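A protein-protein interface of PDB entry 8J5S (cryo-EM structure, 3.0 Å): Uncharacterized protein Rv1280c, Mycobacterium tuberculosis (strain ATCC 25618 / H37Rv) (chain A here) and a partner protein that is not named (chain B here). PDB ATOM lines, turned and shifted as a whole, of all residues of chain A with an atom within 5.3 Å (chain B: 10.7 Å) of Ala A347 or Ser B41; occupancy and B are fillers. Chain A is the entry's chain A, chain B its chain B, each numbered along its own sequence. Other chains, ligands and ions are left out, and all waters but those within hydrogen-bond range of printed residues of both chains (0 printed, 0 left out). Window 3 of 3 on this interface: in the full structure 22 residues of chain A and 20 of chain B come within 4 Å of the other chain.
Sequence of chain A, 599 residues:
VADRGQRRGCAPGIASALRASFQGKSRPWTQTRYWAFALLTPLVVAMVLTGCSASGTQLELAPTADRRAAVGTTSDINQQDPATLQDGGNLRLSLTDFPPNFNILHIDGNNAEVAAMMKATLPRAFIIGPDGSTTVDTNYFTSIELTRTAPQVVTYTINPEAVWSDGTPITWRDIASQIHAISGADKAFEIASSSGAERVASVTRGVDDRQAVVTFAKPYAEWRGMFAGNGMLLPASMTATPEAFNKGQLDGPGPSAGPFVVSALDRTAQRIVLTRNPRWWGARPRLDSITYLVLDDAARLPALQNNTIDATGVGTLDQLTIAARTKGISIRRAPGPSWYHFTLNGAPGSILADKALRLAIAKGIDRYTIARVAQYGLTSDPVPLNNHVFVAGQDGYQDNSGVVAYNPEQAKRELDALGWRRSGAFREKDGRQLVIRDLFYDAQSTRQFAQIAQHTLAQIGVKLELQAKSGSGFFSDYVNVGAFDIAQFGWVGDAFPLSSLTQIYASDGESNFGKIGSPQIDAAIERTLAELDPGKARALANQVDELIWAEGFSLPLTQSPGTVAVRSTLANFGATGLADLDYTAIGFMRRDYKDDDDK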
ATOM      1  N   ASN A 345     -22.651  13.073  -2.300  1.00  0.00           N
ATOM      2  CA  ASN A 345     -23.247  14.262  -2.964  1.00  0.00           C
ATOM      3  C   ASN A 345     -23.707  13.861  -4.369  1.00  0.00           C
ATOM      4  O   ASN A 345     -22.836  13.589  -5.217  1.00  0.00           O
ATOM      5  CB  ASN A 345     -22.264  15.435  -2.987  1.00  0.00           C
ATOM      6  CG  ASN A 345     -22.939  16.781  -3.140  1.00  0.00           C
ATOM      7  OD1 ASN A 345     -24.155  16.857  -3.303  1.00  0.00           O
ATOM      8  ND2 ASN A 345     -22.158  17.847  -3.090  1.00  0.00           N
ATOM      9  N   GLY A 346     -25.022  13.807  -4.594  1.00  0.00           N
ATOM     10  CA  GLY A 346     -25.559  13.466  -5.926  1.00  0.00           C
ATOM     11  C   GLY A 346     -26.013  14.709  -6.668  1.00  0.00           C
ATOM     12  O   GLY A 346     -26.551  14.567  -7.783  1.00  0.00           O
ATOM     13  N   ALA A 347     -25.803  15.886  -6.071  1.00  0.00           N
ATOM     14  CA  ALA A 347     -26.195  17.159  -6.718  1.00  0.00           C
ATOM     15  C   ALA A 347     -25.483  17.278  -8.069  1.00  0.00           C
ATOM     16  O   ALA A 347     -24.283  16.947  -8.139  1.00  0.00           O
ATOM     17  CB  ALA A 347     -25.861  18.318  -5.813  1.00  0.00           C
ATOM     18  N   PRO A 348     -26.165  17.738  -9.142  1.00  0.00           N
ATOM     19  CA  PRO A 348     -25.553  17.821 -10.468  1.00  0.00           C
ATOM     20  C   PRO A 348     -24.209  18.556 -10.386  1.00  0.00           C
ATOM     21  O   PRO A 348     -24.162  19.601  -9.767  1.00  0.00           O
ATOM     22  CB  PRO A 348     -26.563  18.652 -11.269  1.00  0.00           C
ATOM     23  CG  PRO A 348     -27.888  18.355 -10.604  1.00  0.00           C
ATOM     24  CD  PRO A 348     -27.556  18.196  -9.135  1.00  0.00           C
ATOM     25  N   GLY A 349     -23.167  18.008 -11.017  1.00  0.00           N
ATOM     26  CA  GLY A 349     -21.823  18.613 -10.936  1.00  0.00           C
ATOM     27  C   GLY A 349     -20.893  17.761 -10.090  1.00  0.00           C
ATOM     28  O   GLY A 349     -19.666  17.971 -10.171  1.00  0.00           O
ATOM     29  N   SER A 350     -21.452  16.829  -9.311  1.00  0.00           N
ATOM     30  CA  SER A 350     -20.621  15.906  -8.494  1.00  0.00           C
ATOM     31  C   SER A 350     -20.223  14.694  -9.340  1.00  0.00           C
ATOM     32  O   SER A 350     -21.088  14.183 -10.075  1.00  0.00           O
ATOM     33  CB  SER A 350     -21.352  15.478  -7.252  1.00  0.00           C
ATOM     34  OG  SER A 350     -20.582  14.543  -6.510  1.00  0.00           O
ATOM     35  N   ALA A 353     -22.820  12.168  -9.332  1.00  0.00           N
ATOM     36  CA  ALA A 353     -24.189  12.405  -9.766  1.00  0.00           C
ATOM     37  C   ALA A 353     -24.787  11.180 -10.435  1.00  0.00           C
ATOM     38  O   ALA A 353     -26.008  11.113 -10.607  1.00  0.00           O
ATOM     39  CB  ALA A 353     -24.238  13.599 -10.712  1.00  0.00           C
ATOM     40  N   ARG A 437     -13.314  13.211  -3.351  1.00  0.00           N
ATOM     41  CA  ARG A 437     -12.857  13.962  -2.196  1.00  0.00           C
ATOM     42  C   ARG A 437     -13.624  13.532  -0.956  1.00  0.00           C
ATOM     43  O   ARG A 437     -14.848  13.412  -0.988  1.00  0.00           O
ATOM     44  CB  ARG A 437     -13.037  15.459  -2.423  1.00  0.00           C
ATOM     45  CG  ARG A 437     -12.361  16.004  -3.659  1.00  0.00           C
ATOM     46  CD  ARG A 437     -12.780  17.441  -3.914  1.00  0.00           C
ATOM     47  NE  ARG A 437     -14.089  17.527  -4.548  1.00  0.00           N
ATOM     48  CZ  ARG A 437     -14.929  18.541  -4.392  1.00  0.00           C
ATOM     49  NH1 ARG A 437     -14.599  19.562  -3.618  1.00  0.00           N
ATOM     50  NH2 ARG A 437     -16.101  18.534  -5.006  1.00  0.00           N
ATOM     51  N   GLY A 482     -22.345  22.271   0.029  1.00  0.00           N
ATOM     52  CA  GLY A 482     -22.100  21.301  -1.012  1.00  0.00           C
ATOM     53  C   GLY A 482     -20.660  21.128  -1.424  1.00  0.00           C
ATOM     54  O   GLY A 482     -20.411  20.607  -2.512  1.00  0.00           O
ATOM     55  N   ALA A 483     -19.707  21.540  -0.597  1.00  0.00           N
ATOM     56  CA  ALA A 483     -18.299  21.523  -0.978  1.00  0.00           C
ATOM     57  C   ALA A 483     -17.639  20.205  -0.581  1.00  0.00           C
ATOM     58  O   ALA A 483     -16.669  20.163   0.167  1.00  0.00           O
ATOM     59  CB  ALA A 483     -17.574  22.710  -0.359  1.00  0.00           C
ATOM     60  N   PHE A 484     -18.184  19.114  -1.111  1.00  0.00           N
ATOM     61  CA  PHE A 484     -17.667  17.786  -0.816  1.00  0.00           C
ATOM     62  C   PHE A 484     -18.139  16.815  -1.884  1.00  0.00           C
ATOM     63  O   PHE A 484     -19.115  17.065  -2.590  1.00  0.00           O
ATOM     64  CB  PHE A 484     -18.107  17.303   0.569  1.00  0.00           C
ATOM     65  CG  PHE A 484     -19.594  17.131   0.716  1.00  0.00           C
ATOM     66  CD1 PHE A 484     -20.202  15.932   0.432  1.00  0.00           C
ATOM     67  CD2 PHE A 484     -20.379  18.169   1.155  1.00  0.00           C
ATOM     68  CE1 PHE A 484     -21.546  15.779   0.567  1.00  0.00           C
ATOM     69  CE2 PHE A 484     -21.731  18.016   1.285  1.00  0.00           C
ATOM     70  CZ  PHE A 484     -22.311  16.817   0.994  1.00  0.00           C
ATOM     71  N   GLY A 514     -26.926  16.331   0.171  1.00  0.00           N
ATOM     72  CA  GLY A 514     -26.422  15.786  -1.070  1.00  0.00           C
ATOM     73  C   GLY A 514     -27.399  15.898  -2.216  1.00  0.00           C
ATOM     74  O   GLY A 514     -27.057  15.598  -3.356  1.00  0.00           O
ATOM     75  N   LYS A 515     -28.620  16.320  -1.919  1.00  0.00           N
ATOM     76  CA  LYS A 515     -29.650  16.552  -2.929  1.00  0.00           C
ATOM     77  C   LYS A 515     -29.948  15.296  -3.741  1.00  0.00           C
ATOM     78  O   LYS A 515     -30.208  15.363  -4.942  1.00  0.00           O
ATOM     79  CB  LYS A 515     -29.268  17.710  -3.849  1.00  0.00           C
ATOM     80  CG  LYS A 515     -29.660  19.071  -3.318  1.00  0.00           C
ATOM     81  CD  LYS A 515     -28.462  19.785  -2.744  1.00  0.00           C
ATOM     82  CE  LYS A 515     -28.782  21.221  -2.406  1.00  0.00           C
ATOM     83  NZ  LYS A 515     -27.582  21.940  -1.906  1.00  0.00           N
ATOM     84  N   ILE A 516     -29.926  14.146  -3.084  1.00  0.00           N
ATOM     85  CA  ILE A 516     -30.328  12.882  -3.690  1.00  0.00           C
ATOM     86  C   ILE A 516     -31.764  12.604  -3.290  1.00  0.00           C
ATOM     87  O   ILE A 516     -32.150  12.817  -2.137  1.00  0.00           O
ATOM     88  CB  ILE A 516     -29.405  11.728  -3.260  1.00  0.00           C
ATOM     89  CG1 ILE A 516     -28.046  11.851  -3.922  1.00  0.00           C
ATOM     90  CG2 ILE A 516     -30.011  10.402  -3.619  1.00  0.00           C
ATOM     91  CD1 ILE A 516     -26.923  11.410  -3.053  1.00  0.00           C
ATOM     92  N   GLU B  35     -10.754  27.898  -4.898  1.00  0.00           N
ATOM     93  CA  GLU B  35     -10.876  26.516  -5.346  1.00  0.00           C
ATOM     94  C   GLU B  35     -11.995  25.792  -4.612  1.00  0.00           C
ATOM     95  O   GLU B  35     -12.848  25.151  -5.234  1.00  0.00           O
ATOM     96  CB  GLU B  35      -9.554  25.788  -5.144  1.00  0.00           C
ATOM     97  CG  GLU B  35      -9.285  24.709  -6.153  1.00  0.00           C
ATOM     98  CD  GLU B  35      -7.842  24.260  -6.136  1.00  0.00           C
ATOM     99  OE1 GLU B  35      -7.170  24.380  -7.184  1.00  0.00           O
ATOM    100  OE2 GLU B  35      -7.380  23.796  -5.071  1.00  0.00           O
ATOM    101  N   SER B  36     -12.009  25.886  -3.286  1.00  0.00           N
ATOM    102  CA  SER B  36     -13.029  25.213  -2.498  1.00  0.00           C
ATOM    103  C   SER B  36     -14.406  25.800  -2.715  1.00  0.00           C
ATOM    104  O   SER B  36     -15.393  25.179  -2.317  1.00  0.00           O
ATOM    105  CB  SER B  36     -12.682  25.277  -1.015  1.00  0.00           C
ATOM    106  OG  SER B  36     -13.801  24.922  -0.226  1.00  0.00           O
ATOM    107  N   LEU B  37     -14.456  27.016  -3.252  1.00  0.00           N
ATOM    108  CA  LEU B  37     -15.712  27.710  -3.508  1.00  0.00           C
ATOM    109  C   LEU B  37     -16.197  27.339  -4.896  1.00  0.00           C
ATOM    110  O   LEU B  37     -17.377  27.055  -5.102  1.00  0.00           O
ATOM    111  CB  LEU B  37     -15.518  29.224  -3.402  1.00  0.00           C
ATOM    112  CG  LEU B  37     -16.751  30.108  -3.604  1.00  0.00           C
ATOM    113  CD1 LEU B  37     -16.429  31.561  -3.289  1.00  0.00           C
ATOM    114  CD2 LEU B  37     -17.299  29.970  -5.017  1.00  0.00           C
ATOM    115  N   MET B  38     -15.270  27.342  -5.849  1.00  0.00           N
ATOM    116  CA  MET B  38     -15.576  26.974  -7.223  1.00  0.00           C
ATOM    117  C   MET B  38     -16.011  25.513  -7.283  1.00  0.00           C
ATOM    118  O   MET B  38     -16.940  25.162  -8.011  1.00  0.00           O
ATOM    119  CB  MET B  38     -14.363  27.203  -8.128  1.00  0.00           C
ATOM    120  CG  MET B  38     -13.915  28.653  -8.209  1.00  0.00           C
ATOM    121  SD  MET B  38     -12.539  28.892  -9.349  1.00  0.00           S
ATOM    122  CE  MET B  38     -11.302  27.824  -8.616  1.00  0.00           C
ATOM    123  N   GLN B  39     -15.336  24.628  -6.561  1.00  0.00           N
ATOM    124  CA  GLN B  39     -15.651  23.175  -6.670  1.00  0.00           C
ATOM    125  C   GLN B  39     -16.716  22.800  -5.641  1.00  0.00           C
ATOM    126  O   GLN B  39     -16.397  22.041  -4.733  1.00  0.00           O
ATOM    127  CB  GLN B  39     -14.390  22.328  -6.542  1.00  0.00           C
ATOM    128  CG  GLN B  39     -13.394  22.499  -7.670  1.00  0.00           C
ATOM    129  CD  GLN B  39     -12.065  21.933  -7.244  1.00  0.00           C
ATOM    130  OE1 GLN B  39     -11.964  21.234  -6.241  1.00  0.00           O
ATOM    131  NE2 GLN B  39     -11.026  22.237  -8.003  1.00  0.00           N
ATOM    132  N   ARG B  40     -17.904  23.379  -5.750  1.00  0.00           N
ATOM    133  CA  ARG B  40     -19.052  23.042  -4.890  1.00  0.00           C
ATOM    134  C   ARG B  40     -19.921  22.253  -5.846  1.00  0.00           C
ATOM    135  O   ARG B  40     -19.825  22.517  -7.034  1.00  0.00           O
ATOM    136  CB  ARG B  40     -19.749  24.305  -4.407  1.00  0.00           C
ATOM    137  CG  ARG B  40     -19.717  24.485  -2.902  1.00  0.00           C
ATOM    138  CD  ARG B  40     -18.809  25.621  -2.504  1.00  0.00           C
ATOM    139  NE  ARG B  40     -19.586  26.838  -2.388  1.00  0.00           N
ATOM    140  CZ  ARG B  40     -19.596  27.610  -1.316  1.00  0.00           C
ATOM    141  NH1 ARG B  40     -18.625  27.516  -0.429  1.00  0.00           N
ATOM    142  NH2 ARG B  40     -20.578  28.472  -1.137  1.00  0.00           N
ATOM    143  N   SER B  41     -20.601  21.200  -5.387  1.00  0.00           N
ATOM    144  CA  SER B  41     -21.351  20.383  -6.382  1.00  0.00           C
ATOM    145  C   SER B  41     -22.398  21.260  -7.075  1.00  0.00           C
ATOM    146  O   SER B  41     -22.338  21.346  -8.316  1.00  0.00           O
ATOM    147  CB  SER B  41     -21.945  19.129  -5.804  1.00  0.00           C
ATOM    148  OG  SER B  41     -22.696  18.442  -6.791  1.00  0.00           O
ATOM    149  N   PRO B  42     -23.417  21.839  -6.393  1.00  0.00           N
ATOM    150  CA  PRO B  42     -24.306  22.747  -7.110  1.00  0.00           C
ATOM    151  C   PRO B  42     -23.426  23.967  -7.451  1.00  0.00           C
ATOM    152  O   PRO B  42     -23.465  24.910  -6.710  1.00  0.00           O
ATOM    153  CB  PRO B  42     -25.429  22.997  -6.114  1.00  0.00           C
ATOM    154  CG  PRO B  42     -25.286  21.921  -5.079  1.00  0.00           C
ATOM    155  CD  PRO B  42     -23.798  21.713  -4.978  1.00  0.00           C
ATOM    156  N   ARG B  43     -22.660  23.902  -8.536  1.00  0.00           N
ATOM    157  CA  ARG B  43     -21.667  24.960  -8.828  1.00  0.00           C
ATOM    158  C   ARG B  43     -22.302  26.312  -8.553  1.00  0.00           C
ATOM    159  O   ARG B  43     -23.336  26.601  -9.157  1.00  0.00           O
ATOM    160  CB  ARG B  43     -21.123  24.791 -10.244  1.00  0.00           C
ATOM    161  CG  ARG B  43     -19.659  25.173 -10.387  1.00  0.00           C
ATOM    162  CD  ARG B  43     -18.773  23.974 -10.650  1.00  0.00           C
ATOM    163  NE  ARG B  43     -19.008  22.891  -9.708  1.00  0.00           N
ATOM    164  CZ  ARG B  43     -18.817  21.608  -9.984  1.00  0.00           C
ATOM    165  NH1 ARG B  43     -18.422  20.779  -9.035  1.00  0.00           N
ATOM    166  NH2 ARG B  43     -19.020  21.161 -11.210  1.00  0.00           N
ATOM    167  N   PRO B  44     -21.703  27.138  -7.674  1.00  0.00           N
ATOM    168  CA  PRO B  44     -22.274  28.431  -7.286  1.00  0.00           C
ATOM    169  C   PRO B  44     -22.345  29.394  -8.481  1.00  0.00           C
ATOM    170  O   PRO B  44     -21.481  29.337  -9.341  1.00  0.00           O
ATOM    171  CB  PRO B  44     -21.289  28.942  -6.225  1.00  0.00           C
ATOM    172  CG  PRO B  44     -20.006  28.208  -6.526  1.00  0.00           C
ATOM    173  CD  PRO B  44     -20.453  26.835  -6.977  1.00  0.00           C
ATOM    174  N   PRO B  45     -23.369  30.273  -8.547  1.00  0.00           N
ATOM    175  CA  PRO B  45     -23.500  31.234  -9.659  1.00  0.00           C
ATOM    176  C   PRO B  45     -22.290  32.127 -10.003  1.00  0.00           C
ATOM    177  O   PRO B  45     -21.425  32.223  -9.193  1.00  0.00           O
ATOM    178  CB  PRO B  45     -24.656  32.109  -9.164  1.00  0.00           C
ATOM    179  CG  PRO B  45     -25.479  31.179  -8.314  1.00  0.00           C
ATOM    180  CD  PRO B  45     -24.450  30.361  -7.570  1.00  0.00           C
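OG of Ser B41 lies within hydrogen-bond range of N of Ser A350.
OG of Ser B41 is in hydrogen-bond range of O of Ala A347, at 2.6 Å.
O of Gly A482 sits at hydrogen-bond distance from N of Ser B41, at 2.9 Å.
The guanidinium group of Arg B43 is in hydrogen-bond range of the backbone carbonyl oxygen of Gly A349 (3.3 Å).
The guanidinium group (NH1) of Arg A437 sits at hydrogen-bond distance from the backbone carbonyl oxygen (O) of Gln B39 (3.3 Å).
The backbone carbonyl oxygen (O) of Pro A348 lies close to the backbone carbonyl oxygen (O) of Ser B41 (2.9 Å).
Asn A345 touches just one residue of chain B: Ser B41.
No residue of chain B comes within 4 Å of Gly A346.
Ala A347 touches just these residues of chain B: Ser B41 and Pro B42.
Printed residues of chain B within 4 Å of Pro A348: Ser B41.
Gly A349 touches just these residues of chain B: Ser B41 and Arg B43.
No residue of chain B comes within 4 Å of Ala A353.
No residue of chain B comes within 4 Å of Gly A514.
Lys A515 touches one residue of chain B.
Of the printed residues of chain A, Ser B36 touches Ala A483 (3.8 Å).
Of the printed residues of chain A, Gln B39 touches Arg A437.
Ser B41 touches just these residues of chain A: Asn A345 (3.0 Å), Ala A347 (2.6 Å), Pro A348 (2.9 Å), Gly A349 (3.8 Å), Ser A350 (3.2 Å) and Gly A482 (2.9 Å).
Printed residues of chain A within 4 Å of Arg B43: Gly A349 (3.3 Å).
The nearest residue of chain A that does not touch Ser B41 is Phe A484 (4.8 Å).
The nearest printed residue of chain B that does not touch Ala A483 is Gln B39 (4.2 Å).
CB of Ser B41 touches ND2 of Asn A345, at 3.0 Å.
Pro B42 touches Ala A347.
Ser B41 touches Gly A349.
CA of Arg B40 touches O of Gly A482, at 3.7 Å.
Ser B36 touches Ala A483 (O to CB, 3.8 Å).
CG of Arg B40 touches N of Ala A483, 3.7 Å away.
Lys A515 touches Pro B42.
Of the 14 printed residues of chain A, 9 touch a printed residue of chain B.
Hydrophobic or aromatic side chains of chain A that line the printed part of chain B: Ala A347 and Ala A483.
Hydrophobic or aromatic side chains of chain B that line the printed part of chain A: Pro B42.
The backbone NH (N) of Ala A347 lies within hydrogen-bond range of the backbone carbonyl oxygen (O) of Gly A514 (3.0 Å).
The side-chain amide nitrogen (ND2) of Asn A345 is in hydrogen-bond range of the backbone carbonyl oxygen (O) of Gly A482, at 3.3 Å.
O of Phe A484 lies within hydrogen-bond range of ND2 of Asn A345, at 3.2 Å.
O of Arg B40 sits at hydrogen-bond distance from NE of Arg B43 (2.8 Å).
The side-chain amide oxygen (OD1) of Asn A345 lies within hydrogen-bond range of the backbone NH (N) of Ala A347.
O of Gly A514 sits close to OD1 of Asn A345.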
